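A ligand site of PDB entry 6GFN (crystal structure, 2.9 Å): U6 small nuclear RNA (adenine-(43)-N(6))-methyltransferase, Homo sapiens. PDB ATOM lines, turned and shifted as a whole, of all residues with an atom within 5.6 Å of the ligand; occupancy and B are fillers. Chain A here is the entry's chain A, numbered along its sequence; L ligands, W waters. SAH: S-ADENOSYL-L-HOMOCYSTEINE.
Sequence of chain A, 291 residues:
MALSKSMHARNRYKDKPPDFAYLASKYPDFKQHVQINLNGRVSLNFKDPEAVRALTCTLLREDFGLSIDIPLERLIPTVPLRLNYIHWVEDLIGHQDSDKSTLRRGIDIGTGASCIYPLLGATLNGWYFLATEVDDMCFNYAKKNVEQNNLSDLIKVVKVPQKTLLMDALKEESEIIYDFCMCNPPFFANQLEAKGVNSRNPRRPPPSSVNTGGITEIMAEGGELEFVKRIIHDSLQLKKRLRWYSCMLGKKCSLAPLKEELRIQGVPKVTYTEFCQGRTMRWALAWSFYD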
ATOM      1  N   LEU A  75      -4.869  10.665  19.018  1.00  0.00           N
ATOM      2  CA  LEU A  75      -3.534  11.051  19.485  1.00  0.00           C
ATOM      3  C   LEU A  75      -2.886  12.093  18.599  1.00  0.00           C
ATOM      4  O   LEU A  75      -2.879  11.942  17.363  1.00  0.00           O
ATOM      5  CB  LEU A  75      -2.610   9.807  19.582  1.00  0.00           C
ATOM      6  CG  LEU A  75      -1.103  10.043  19.810  1.00  0.00           C
ATOM      7  CD1 LEU A  75      -0.813  10.476  21.224  1.00  0.00           C
ATOM      8  CD2 LEU A  75      -0.293   8.803  19.501  1.00  0.00           C
ATOM      9  N   PRO A  77       0.667  13.497  17.612  1.00  0.00           N
ATOM     10  CA  PRO A  77       2.083  13.163  17.778  1.00  0.00           C
ATOM     11  C   PRO A  77       2.929  14.395  18.040  1.00  0.00           C
ATOM     12  O   PRO A  77       2.512  15.516  17.741  1.00  0.00           O
ATOM     13  CB  PRO A  77       2.455  12.490  16.456  1.00  0.00           C
ATOM     14  CG  PRO A  77       1.551  13.094  15.465  1.00  0.00           C
ATOM     15  CD  PRO A  77       0.281  13.499  16.185  1.00  0.00           C
ATOM     16  N   ARG A  82       9.150  11.767  17.462  1.00  0.00           N
ATOM     17  CA  ARG A  82       8.905  10.722  16.452  1.00  0.00           C
ATOM     18  C   ARG A  82      10.090  10.646  15.501  1.00  0.00           C
ATOM     19  O   ARG A  82      10.451   9.546  15.047  1.00  0.00           O
ATOM     20  CB  ARG A  82       7.604  10.984  15.643  1.00  0.00           C
ATOM     21  CG  ARG A  82       6.295  11.085  16.449  1.00  0.00           C
ATOM     22  CD  ARG A  82       5.787   9.769  17.028  1.00  0.00           C
ATOM     23  NE  ARG A  82       4.532   9.936  17.768  1.00  0.00           N
ATOM     24  CZ  ARG A  82       4.431  10.390  19.026  1.00  0.00           C
ATOM     25  NH1 ARG A  82       5.513  10.758  19.695  1.00  0.00           N
ATOM     26  NH2 ARG A  82       3.234  10.492  19.604  1.00  0.00           N
ATOM     27  N   ASP A 108       4.570   0.007   9.179  1.00  0.00           N
ATOM     28  CA  ASP A 108       4.188   0.804  10.342  1.00  0.00           C
ATOM     29  C   ASP A 108       2.917   0.211  10.989  1.00  0.00           C
ATOM     30  O   ASP A 108       1.803   0.360  10.469  1.00  0.00           O
ATOM     31  CB  ASP A 108       4.088   2.313  10.053  1.00  0.00           C
ATOM     32  CG  ASP A 108       3.896   3.159  11.297  1.00  0.00           C
ATOM     33  OD1 ASP A 108       4.376   2.743  12.375  1.00  0.00           O
ATOM     34  OD2 ASP A 108       3.260   4.233  11.193  1.00  0.00           O
ATOM     35  N   ILE A 109       3.130  -0.542  12.084  1.00  0.00           N
ATOM     36  CA  ILE A 109       2.118  -1.190  12.900  1.00  0.00           C
ATOM     37  C   ILE A 109       1.494  -0.084  13.743  1.00  0.00           C
ATOM     38  O   ILE A 109       2.108   0.421  14.683  1.00  0.00           O
ATOM     39  CB  ILE A 109       2.756  -2.327  13.730  1.00  0.00           C
ATOM     40  CG1 ILE A 109       3.318  -3.437  12.814  1.00  0.00           C
ATOM     41  CG2 ILE A 109       1.764  -2.901  14.734  1.00  0.00           C
ATOM     42  CD1 ILE A 109       4.794  -3.285  12.350  1.00  0.00           C
ATOM     43  N   GLY A 110       0.297   0.325  13.326  1.00  0.00           N
ATOM     44  CA  GLY A 110      -0.452   1.392  13.964  1.00  0.00           C
ATOM     45  C   GLY A 110       0.037   2.733  13.505  1.00  0.00           C
ATOM     46  O   GLY A 110       0.863   3.352  14.171  1.00  0.00           O
ATOM     47  N   THR A 111      -0.425   3.184  12.346  1.00  0.00           N
ATOM     48  CA  THR A 111       0.062   4.409  11.752  1.00  0.00           C
ATOM     49  C   THR A 111      -0.554   5.689  12.384  1.00  0.00           C
ATOM     50  O   THR A 111       0.041   6.768  12.264  1.00  0.00           O
ATOM     51  CB  THR A 111      -0.077   4.313  10.228  1.00  0.00           C
ATOM     52  OG1 THR A 111       0.989   5.006   9.593  1.00  0.00           O
ATOM     53  CG2 THR A 111      -1.459   4.752   9.695  1.00  0.00           C
ATOM     54  N   GLY A 112      -1.709   5.571  13.032  1.00  0.00           N
ATOM     55  CA  GLY A 112      -2.416   6.710  13.610  1.00  0.00           C
ATOM     56  C   GLY A 112      -3.029   7.624  12.563  1.00  0.00           C
ATOM     57  O   GLY A 112      -2.749   7.481  11.369  1.00  0.00           O
ATOM     58  N   ALA A 113      -3.889   8.580  12.991  1.00  0.00           N
ATOM     59  CA  ALA A 113      -4.561   9.536  12.091  1.00  0.00           C
ATOM     60  C   ALA A 113      -3.548  10.389  11.294  1.00  0.00           C
ATOM     61  O   ALA A 113      -3.767  10.669  10.115  1.00  0.00           O
ATOM     62  CB  ALA A 113      -5.491  10.436  12.888  1.00  0.00           C
ATOM     63  N   SER A 114      -2.432  10.728  11.956  1.00  0.00           N
ATOM     64  CA  SER A 114      -1.291  11.495  11.456  1.00  0.00           C
ATOM     65  C   SER A 114      -0.582  10.840  10.294  1.00  0.00           C
ATOM     66  O   SER A 114      -0.265  11.514   9.315  1.00  0.00           O
ATOM     67  CB  SER A 114      -0.285  11.712  12.591  1.00  0.00           C
ATOM     68  OG  SER A 114      -0.050  10.544  13.362  1.00  0.00           O
ATOM     69  N   ILE A 116       2.297   9.720  10.707  1.00  0.00           N
ATOM     70  CA  ILE A 116       3.513  10.472  10.936  1.00  0.00           C
ATOM     71  C   ILE A 116       4.759   9.731  10.472  1.00  0.00           C
ATOM     72  O   ILE A 116       5.449  10.303   9.629  1.00  0.00           O
ATOM     73  CB  ILE A 116       3.605  11.023  12.401  1.00  0.00           C
ATOM     74  CG1 ILE A 116       4.728  12.056  12.528  1.00  0.00           C
ATOM     75  CG2 ILE A 116       3.687   9.920  13.479  1.00  0.00           C
ATOM     76  CD1 ILE A 116       4.462  13.275  11.874  1.00  0.00           C
ATOM     77  N   TYR A 117       5.044   8.494  10.956  1.00  0.00           N
ATOM     78  CA  TYR A 117       6.245   7.747  10.553  1.00  0.00           C
ATOM     79  C   TYR A 117       6.333   7.543   9.044  1.00  0.00           C
ATOM     80  O   TYR A 117       7.336   7.985   8.476  1.00  0.00           O
ATOM     81  CB  TYR A 117       6.453   6.406  11.307  1.00  0.00           C
ATOM     82  CG  TYR A 117       6.650   6.529  12.802  1.00  0.00           C
ATOM     83  CD1 TYR A 117       7.627   7.371  13.341  1.00  0.00           C
ATOM     84  CD2 TYR A 117       5.902   5.752  13.692  1.00  0.00           C
ATOM     85  CE1 TYR A 117       7.809   7.485  14.715  1.00  0.00           C
ATOM     86  CE2 TYR A 117       6.097   5.840  15.069  1.00  0.00           C
ATOM     87  CZ  TYR A 117       7.043   6.708  15.579  1.00  0.00           C
ATOM     88  OH  TYR A 117       7.234   6.780  16.941  1.00  0.00           O
ATOM     89  N   THR A 132      -0.397   0.175   8.720  1.00  0.00           N
ATOM     90  CA  THR A 132      -1.557  -0.629   9.171  1.00  0.00           C
ATOM     91  C   THR A 132      -2.350   0.153  10.237  1.00  0.00           C
ATOM     92  O   THR A 132      -1.766   0.959  10.951  1.00  0.00           O
ATOM     93  CB  THR A 132      -1.197  -2.083   9.588  1.00  0.00           C
ATOM     94  OG1 THR A 132      -0.853  -2.189  10.981  1.00  0.00           O
ATOM     95  CG2 THR A 132      -0.116  -2.711   8.717  1.00  0.00           C
ATOM     96  N   GLU A 133      -3.672  -0.073  10.299  1.00  0.00           N
ATOM     97  CA  GLU A 133      -4.560   0.583  11.259  1.00  0.00           C
ATOM     98  C   GLU A 133      -5.797  -0.252  11.561  1.00  0.00           C
ATOM     99  O   GLU A 133      -6.392  -0.814  10.631  1.00  0.00           O
ATOM    100  CB  GLU A 133      -5.018   1.953  10.723  1.00  0.00           C
ATOM    101  CG  GLU A 133      -4.469   3.161  11.474  1.00  0.00           C
ATOM    102  CD  GLU A 133      -4.456   3.125  12.995  1.00  0.00           C
ATOM    103  OE1 GLU A 133      -5.510   2.807  13.605  1.00  0.00           O
ATOM    104  OE2 GLU A 133      -3.397   3.439  13.578  1.00  0.00           O
ATOM    105  N   VAL A 134      -6.219  -0.318  12.848  1.00  0.00           N
ATOM    106  CA  VAL A 134      -7.453  -1.021  13.218  1.00  0.00           C
ATOM    107  C   VAL A 134      -8.620  -0.025  13.343  1.00  0.00           C
ATOM    108  O   VAL A 134      -9.748  -0.383  13.005  1.00  0.00           O
ATOM    109  CB  VAL A 134      -7.354  -1.976  14.449  1.00  0.00           C
ATOM    110  CG1 VAL A 134      -6.382  -3.117  14.195  1.00  0.00           C
ATOM    111  CG2 VAL A 134      -7.019  -1.230  15.735  1.00  0.00           C
ATOM    112  N   ASP A 135      -8.315   1.222  13.805  1.00  0.00           N
ATOM    113  CA  ASP A 135      -9.263   2.316  14.027  1.00  0.00           C
ATOM    114  C   ASP A 135      -9.686   2.975  12.722  1.00  0.00           C
ATOM    115  O   ASP A 135      -8.834   3.447  11.973  1.00  0.00           O
ATOM    116  CB  ASP A 135      -8.646   3.352  14.972  1.00  0.00           C
ATOM    117  CG  ASP A 135      -9.623   4.362  15.527  1.00  0.00           C
ATOM    118  OD1 ASP A 135     -10.050   5.254  14.770  1.00  0.00           O
ATOM    119  OD2 ASP A 135      -9.947   4.271  16.735  1.00  0.00           O
ATOM    120  N   CYS A 138      -8.828   6.807  12.446  1.00  0.00           N
ATOM    121  CA  CYS A 138      -7.403   6.873  12.172  1.00  0.00           C
ATOM    122  C   CYS A 138      -7.100   6.514  10.725  1.00  0.00           C
ATOM    123  O   CYS A 138      -6.416   7.280  10.052  1.00  0.00           O
ATOM    124  CB  CYS A 138      -6.628   6.000  13.142  1.00  0.00           C
ATOM    125  SG  CYS A 138      -6.475   6.680  14.813  1.00  0.00           S
ATOM    126  N   VAL A 160      -6.963  -3.067   9.097  1.00  0.00           N
ATOM    127  CA  VAL A 160      -6.739  -4.457   9.491  1.00  0.00           C
ATOM    128  C   VAL A 160      -7.649  -4.915  10.683  1.00  0.00           C
ATOM    129  O   VAL A 160      -8.095  -4.064  11.454  1.00  0.00           O
ATOM    130  CB  VAL A 160      -5.225  -4.731   9.761  1.00  0.00           C
ATOM    131  CG1 VAL A 160      -4.414  -4.659   8.478  1.00  0.00           C
ATOM    132  CG2 VAL A 160      -4.651  -3.785  10.810  1.00  0.00           C
ATOM    133  N   PRO A 161      -7.946  -6.257  10.825  1.00  0.00           N
ATOM    134  CA  PRO A 161      -8.769  -6.732  11.965  1.00  0.00           C
ATOM    135  C   PRO A 161      -8.065  -6.524  13.312  1.00  0.00           C
ATOM    136  O   PRO A 161      -6.848  -6.333  13.319  1.00  0.00           O
ATOM    137  CB  PRO A 161      -8.921  -8.232  11.694  1.00  0.00           C
ATOM    138  CG  PRO A 161      -8.530  -8.419  10.278  1.00  0.00           C
ATOM    139  CD  PRO A 161      -7.513  -7.391   9.987  1.00  0.00           C
ATOM    140  N   GLN A 162      -8.807  -6.588  14.437  1.00  0.00           N
ATOM    141  CA  GLN A 162      -8.246  -6.307  15.774  1.00  0.00           C
ATOM    142  C   GLN A 162      -7.138  -7.264  16.238  1.00  0.00           C
ATOM    143  O   GLN A 162      -6.045  -6.784  16.622  1.00  0.00           O
ATOM    144  CB  GLN A 162      -9.351  -6.178  16.853  1.00  0.00           C
ATOM    145  CG  GLN A 162      -8.872  -5.632  18.220  1.00  0.00           C
ATOM    146  CD  GLN A 162      -8.169  -4.278  18.167  1.00  0.00           C
ATOM    147  OE1 GLN A 162      -6.928  -4.186  18.185  1.00  0.00           O
ATOM    148  NE2 GLN A 162      -8.945  -3.201  18.125  1.00  0.00           N
ATOM    149  N   LYS A 163      -7.384  -8.584  16.225  1.00  0.00           N
ATOM    150  CA  LYS A 163      -6.410  -9.576  16.679  1.00  0.00           C
ATOM    151  C   LYS A 163      -5.142  -9.683  15.791  1.00  0.00           C
ATOM    152  O   LYS A 163      -4.142 -10.234  16.247  1.00  0.00           O
ATOM    153  CB  LYS A 163      -7.081 -10.948  16.841  1.00  0.00           C
ATOM    154  N   THR A 164      -5.184  -9.127  14.558  1.00  0.00           N
ATOM    155  CA  THR A 164      -4.064  -9.215  13.599  1.00  0.00           C
ATOM    156  C   THR A 164      -2.947  -8.201  13.796  1.00  0.00           C
ATOM    157  O   THR A 164      -3.188  -7.025  14.063  1.00  0.00           O
ATOM    158  CB  THR A 164      -4.549  -9.154  12.142  1.00  0.00           C
ATOM    159  OG1 THR A 164      -4.876  -7.813  11.774  1.00  0.00           O
ATOM    160  CG2 THR A 164      -5.682 -10.131  11.833  1.00  0.00           C
ATOM    161  N   LEU A 165      -1.702  -8.689  13.621  1.00  0.00           N
ATOM    162  CA  LEU A 165      -0.460  -7.915  13.697  1.00  0.00           C
ATOM    163  C   LEU A 165       0.403  -8.197  12.433  1.00  0.00           C
ATOM    164  O   LEU A 165      -0.155  -8.527  11.387  1.00  0.00           O
ATOM    165  CB  LEU A 165       0.277  -8.210  15.033  1.00  0.00           C
ATOM    166  CG  LEU A 165       1.016  -7.047  15.712  1.00  0.00           C
ATOM    167  CD1 LEU A 165       0.069  -5.996  16.187  1.00  0.00           C
ATOM    168  CD2 LEU A 165       1.757  -7.533  16.914  1.00  0.00           C
ATOM    169  N   ASN A 184       4.665   1.994  17.374  1.00  0.00           N
ATOM    170  CA  ASN A 184       4.525   2.816  18.565  1.00  0.00           C
ATOM    171  C   ASN A 184       3.339   2.258  19.357  1.00  0.00           C
ATOM    172  O   ASN A 184       2.198   2.703  19.135  1.00  0.00           O
ATOM    173  CB  ASN A 184       4.369   4.302  18.219  1.00  0.00           C
ATOM    174  CG  ASN A 184       4.405   5.203  19.417  1.00  0.00           C
ATOM    175  OD1 ASN A 184       5.304   5.123  20.266  1.00  0.00           O
ATOM    176  ND2 ASN A 184       3.433   6.092  19.513  1.00  0.00           N
ATOM    177  N   PRO A 185       3.566   1.230  20.224  1.00  0.00           N
ATOM    178  CA  PRO A 185       2.462   0.619  20.968  1.00  0.00           C
ATOM    179  C   PRO A 185       1.544   1.577  21.725  1.00  0.00           C
ATOM    180  O   PRO A 185       2.022   2.494  22.395  1.00  0.00           O
ATOM    181  CB  PRO A 185       3.162  -0.328  21.933  1.00  0.00           C
ATOM    182  CG  PRO A 185       4.395  -0.692  21.242  1.00  0.00           C
ATOM    183  CD  PRO A 185       4.837   0.544  20.537  1.00  0.00           C
ATOM    184  N   PRO A 186       0.207   1.359  21.602  1.00  0.00           N
ATOM    185  CA  PRO A 186      -0.733   2.227  22.344  1.00  0.00           C
ATOM    186  C   PRO A 186      -0.822   1.831  23.826  1.00  0.00           C
ATOM    187  O   PRO A 186      -0.762   0.632  24.141  1.00  0.00           O
ATOM    188  CB  PRO A 186      -2.060   2.019  21.592  1.00  0.00           C
ATOM    189  CG  PRO A 186      -1.925   0.681  20.905  1.00  0.00           C
ATOM    190  CD  PRO A 186      -0.484   0.293  20.850  1.00  0.00           C
ATOM    191  N   PHE A 227       1.838  -6.434  24.157  1.00  0.00           N
ATOM    192  CA  PHE A 227       1.819  -6.019  22.737  1.00  0.00           C
ATOM    193  C   PHE A 227       3.111  -6.369  22.009  1.00  0.00           C
ATOM    194  O   PHE A 227       3.064  -7.056  20.988  1.00  0.00           O
ATOM    195  CB  PHE A 227       1.465  -4.529  22.555  1.00  0.00           C
ATOM    196  CG  PHE A 227       1.131  -4.117  21.127  1.00  0.00           C
ATOM    197  CD1 PHE A 227      -0.138  -4.307  20.599  1.00  0.00           C
ATOM    198  CD2 PHE A 227       2.080  -3.499  20.332  1.00  0.00           C
ATOM    199  CE1 PHE A 227      -0.444  -3.902  19.301  1.00  0.00           C
ATOM    200  CE2 PHE A 227       1.775  -3.094  19.034  1.00  0.00           C
ATOM    201  CZ  PHE A 227       0.511  -3.290  18.529  1.00  0.00           C
ATOM    202  N   ARG A 230       3.580  -9.929  21.273  1.00  0.00           N
ATOM    203  CA  ARG A 230       2.847 -10.319  20.067  1.00  0.00           C
ATOM    204  C   ARG A 230       3.715  -9.976  18.833  1.00  0.00           C
ATOM    205  O   ARG A 230       3.715 -10.746  17.865  1.00  0.00           O
ATOM    206  CB  ARG A 230       1.479  -9.612  20.001  1.00  0.00           C
ATOM    207  CG  ARG A 230       0.255 -10.518  20.202  1.00  0.00           C
ATOM    208  CD  ARG A 230      -1.072  -9.732  20.169  1.00  0.00           C
ATOM    209  NE  ARG A 230      -1.510  -9.401  18.801  1.00  0.00           N
ATOM    210  CZ  ARG A 230      -2.177  -8.298  18.465  1.00  0.00           C
ATOM    211  NH1 ARG A 230      -2.494  -7.390  19.384  1.00  0.00           N
ATOM    212  NH2 ARG A 230      -2.518  -8.089  17.198  1.00  0.00           N
HETATM  213  N   SAH L   1       2.511   5.870  14.888  1.00  0.00           N
HETATM  214  CA  SAH L   1       1.397   6.712  15.364  1.00  0.00           C
HETATM  215  CB  SAH L   1       0.171   6.060  16.093  1.00  0.00           C
HETATM  216  CG  SAH L   1       0.536   5.044  17.167  1.00  0.00           C
HETATM  217  SD  SAH L   1      -0.950   4.885  18.187  1.00  0.00           S
HETATM  218  C   SAH L   1       1.971   7.905  16.178  1.00  0.00           C
HETATM  219  O   SAH L   1       1.248   8.971  15.980  1.00  0.00           O
HETATM  220  OXT SAH L   1       2.954   7.855  16.888  1.00  0.00           O
HETATM  221  C5' SAH L   1      -1.462   3.162  17.964  1.00  0.00           C
HETATM  222  C4' SAH L   1      -2.361   3.092  16.742  1.00  0.00           C
HETATM  223  O4' SAH L   1      -2.305   1.742  16.232  1.00  0.00           O
HETATM  224  C3' SAH L   1      -3.838   3.441  16.925  1.00  0.00           C
HETATM  225  O3' SAH L   1      -4.292   4.388  15.960  1.00  0.00           O
HETATM  226  C2' SAH L   1      -4.557   2.088  16.843  1.00  0.00           C
HETATM  227  O2' SAH L   1      -5.843   2.209  16.246  1.00  0.00           O
HETATM  228  C1' SAH L   1      -3.605   1.249  15.988  1.00  0.00           C
HETATM  229  N9  SAH L   1      -3.602  -0.184  16.278  1.00  0.00           N
HETATM  230  C8  SAH L   1      -3.839  -0.782  17.495  1.00  0.00           C
HETATM  231  N7  SAH L   1      -3.715  -2.081  17.503  1.00  0.00           N
HETATM  232  C5  SAH L   1      -3.375  -2.374  16.190  1.00  0.00           C
HETATM  233  C6  SAH L   1      -3.087  -3.598  15.533  1.00  0.00           C
HETATM  234  N6  SAH L   1      -3.248  -4.794  16.109  1.00  0.00           N
HETATM  235  N1  SAH L   1      -2.710  -3.534  14.236  1.00  0.00           N
HETATM  236  C2  SAH L   1      -2.674  -2.348  13.623  1.00  0.00           C
HETATM  237  N3  SAH L   1      -2.959  -1.137  14.127  1.00  0.00           N
HETATM  238  C4  SAH L   1      -3.297  -1.227  15.426  1.00  0.00           C
HETATM  239  O   HOH W   1       3.191   6.752  12.088  1.00  0.00           O
HETATM  240  O   HOH W   2       3.672   3.391  15.064  1.00  0.00           O
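CD2 of Leu 75 touches O of the ligand, at 3.8 Å.
Pro 77 touches the ligand (CB to O, 3.8 Å).
Thr 111 touches the ligand.
N of Gly 112 touches CB of the ligand, at 3.6 Å.
Ile 116 touches the ligand.
Tyr 117 touches the ligand.
OG1 of Thr 132 touches C2 of the ligand (3.2 Å).
Val 134 touches the ligand.
Asp 135 touches the ligand.
CG2 of Val 160 touches C2 of the ligand, at 3.7 Å.
Leu 165 touches the ligand (CD1 to N6, 3.5 Å).
CB of Pro 186 touches C5' of the ligand (3.9 Å).
NH2 of Arg 230 touches N6 of the ligand (3.5 Å).
21 residues have an atom within 4 Å of the ligand: Leu 75, Pro 77, Arg 82, Gly 110, Thr 111, Gly 112, Ser 114, Ile 116, Tyr 117, Thr 132, Glu 133, Val 134, Asp 135, Cys 138, Val 160, Gln 162, Thr 164, Leu 165, Asn 184, Pro 186 and Arg 230.
The nearest printed residue that does not touch the ligand is Asp 108 (4.1 Å).
The side-chain hydroxyl (OG1) of Thr 164 lies within hydrogen-bond range of the backbone carbonyl oxygen (O) of Pro 161 (2.9 Å).
The guanidinium group (NH2) of Arg 230 lies within hydrogen-bond range of the backbone carbonyl oxygen (O) of Lys 163, at 2.9 Å.
The backbone NH (N) of Gly 110 lies within hydrogen-bond range of the backbone carbonyl oxygen (O) of Thr 132 (3.2 Å).
O of Thr 164 is in hydrogen-bond range of NH2 of Arg 230 (3.4 Å).
SG of Cys 138 sits at hydrogen-bond distance from N of Ala 113 (3.7 Å).
OD1 of Asp 135 is in hydrogen-bond range of N of Cys 138, 3.1 Å away.
The side-chain carboxylate of Glu 133 is in hydrogen-bond range of the backbone NH of Thr 111, 3.2 Å away.
N of Asp 135 is in hydrogen-bond range of OE1 of Glu 133 (3.2 Å).
Water W1 lies within hydrogen-bond range of OD2 of Asp 108 (2.7 Å), N of Tyr 117 (2.8 Å), N of the ligand (3.0 Å), O of Thr 111 (3.2 Å) and N of Ile 116 (3.4 Å).
OE2 of Glu 133 is in hydrogen-bond range of O3' of the ligand, 2.7 Å away.
An oxygen (O) of the ligand lies within hydrogen-bond range of the side-chain hydroxyl (OG) of Ser 114.
SG of Cys 138 sits at hydrogen-bond distance from O3' of the ligand, 3.4 Å away.
ND2 of Asn 184 sits at hydrogen-bond distance from OXT of the ligand (3.2 Å).
NE of Arg 82 is in salt-bridge range of OXT of the ligand, 2.8 Å away.
O of Gln 162 lies within hydrogen-bond range of N6 of the ligand (3.5 Å).
The backbone carbonyl oxygen of Gly 110 lies within hydrogen-bond range of a nitrogen (N) of the ligand (3.1 Å).
The backbone carbonyl oxygen of Thr 164 lies within hydrogen-bond range of a nitrogen (N6) of the ligand (3.0 Å).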
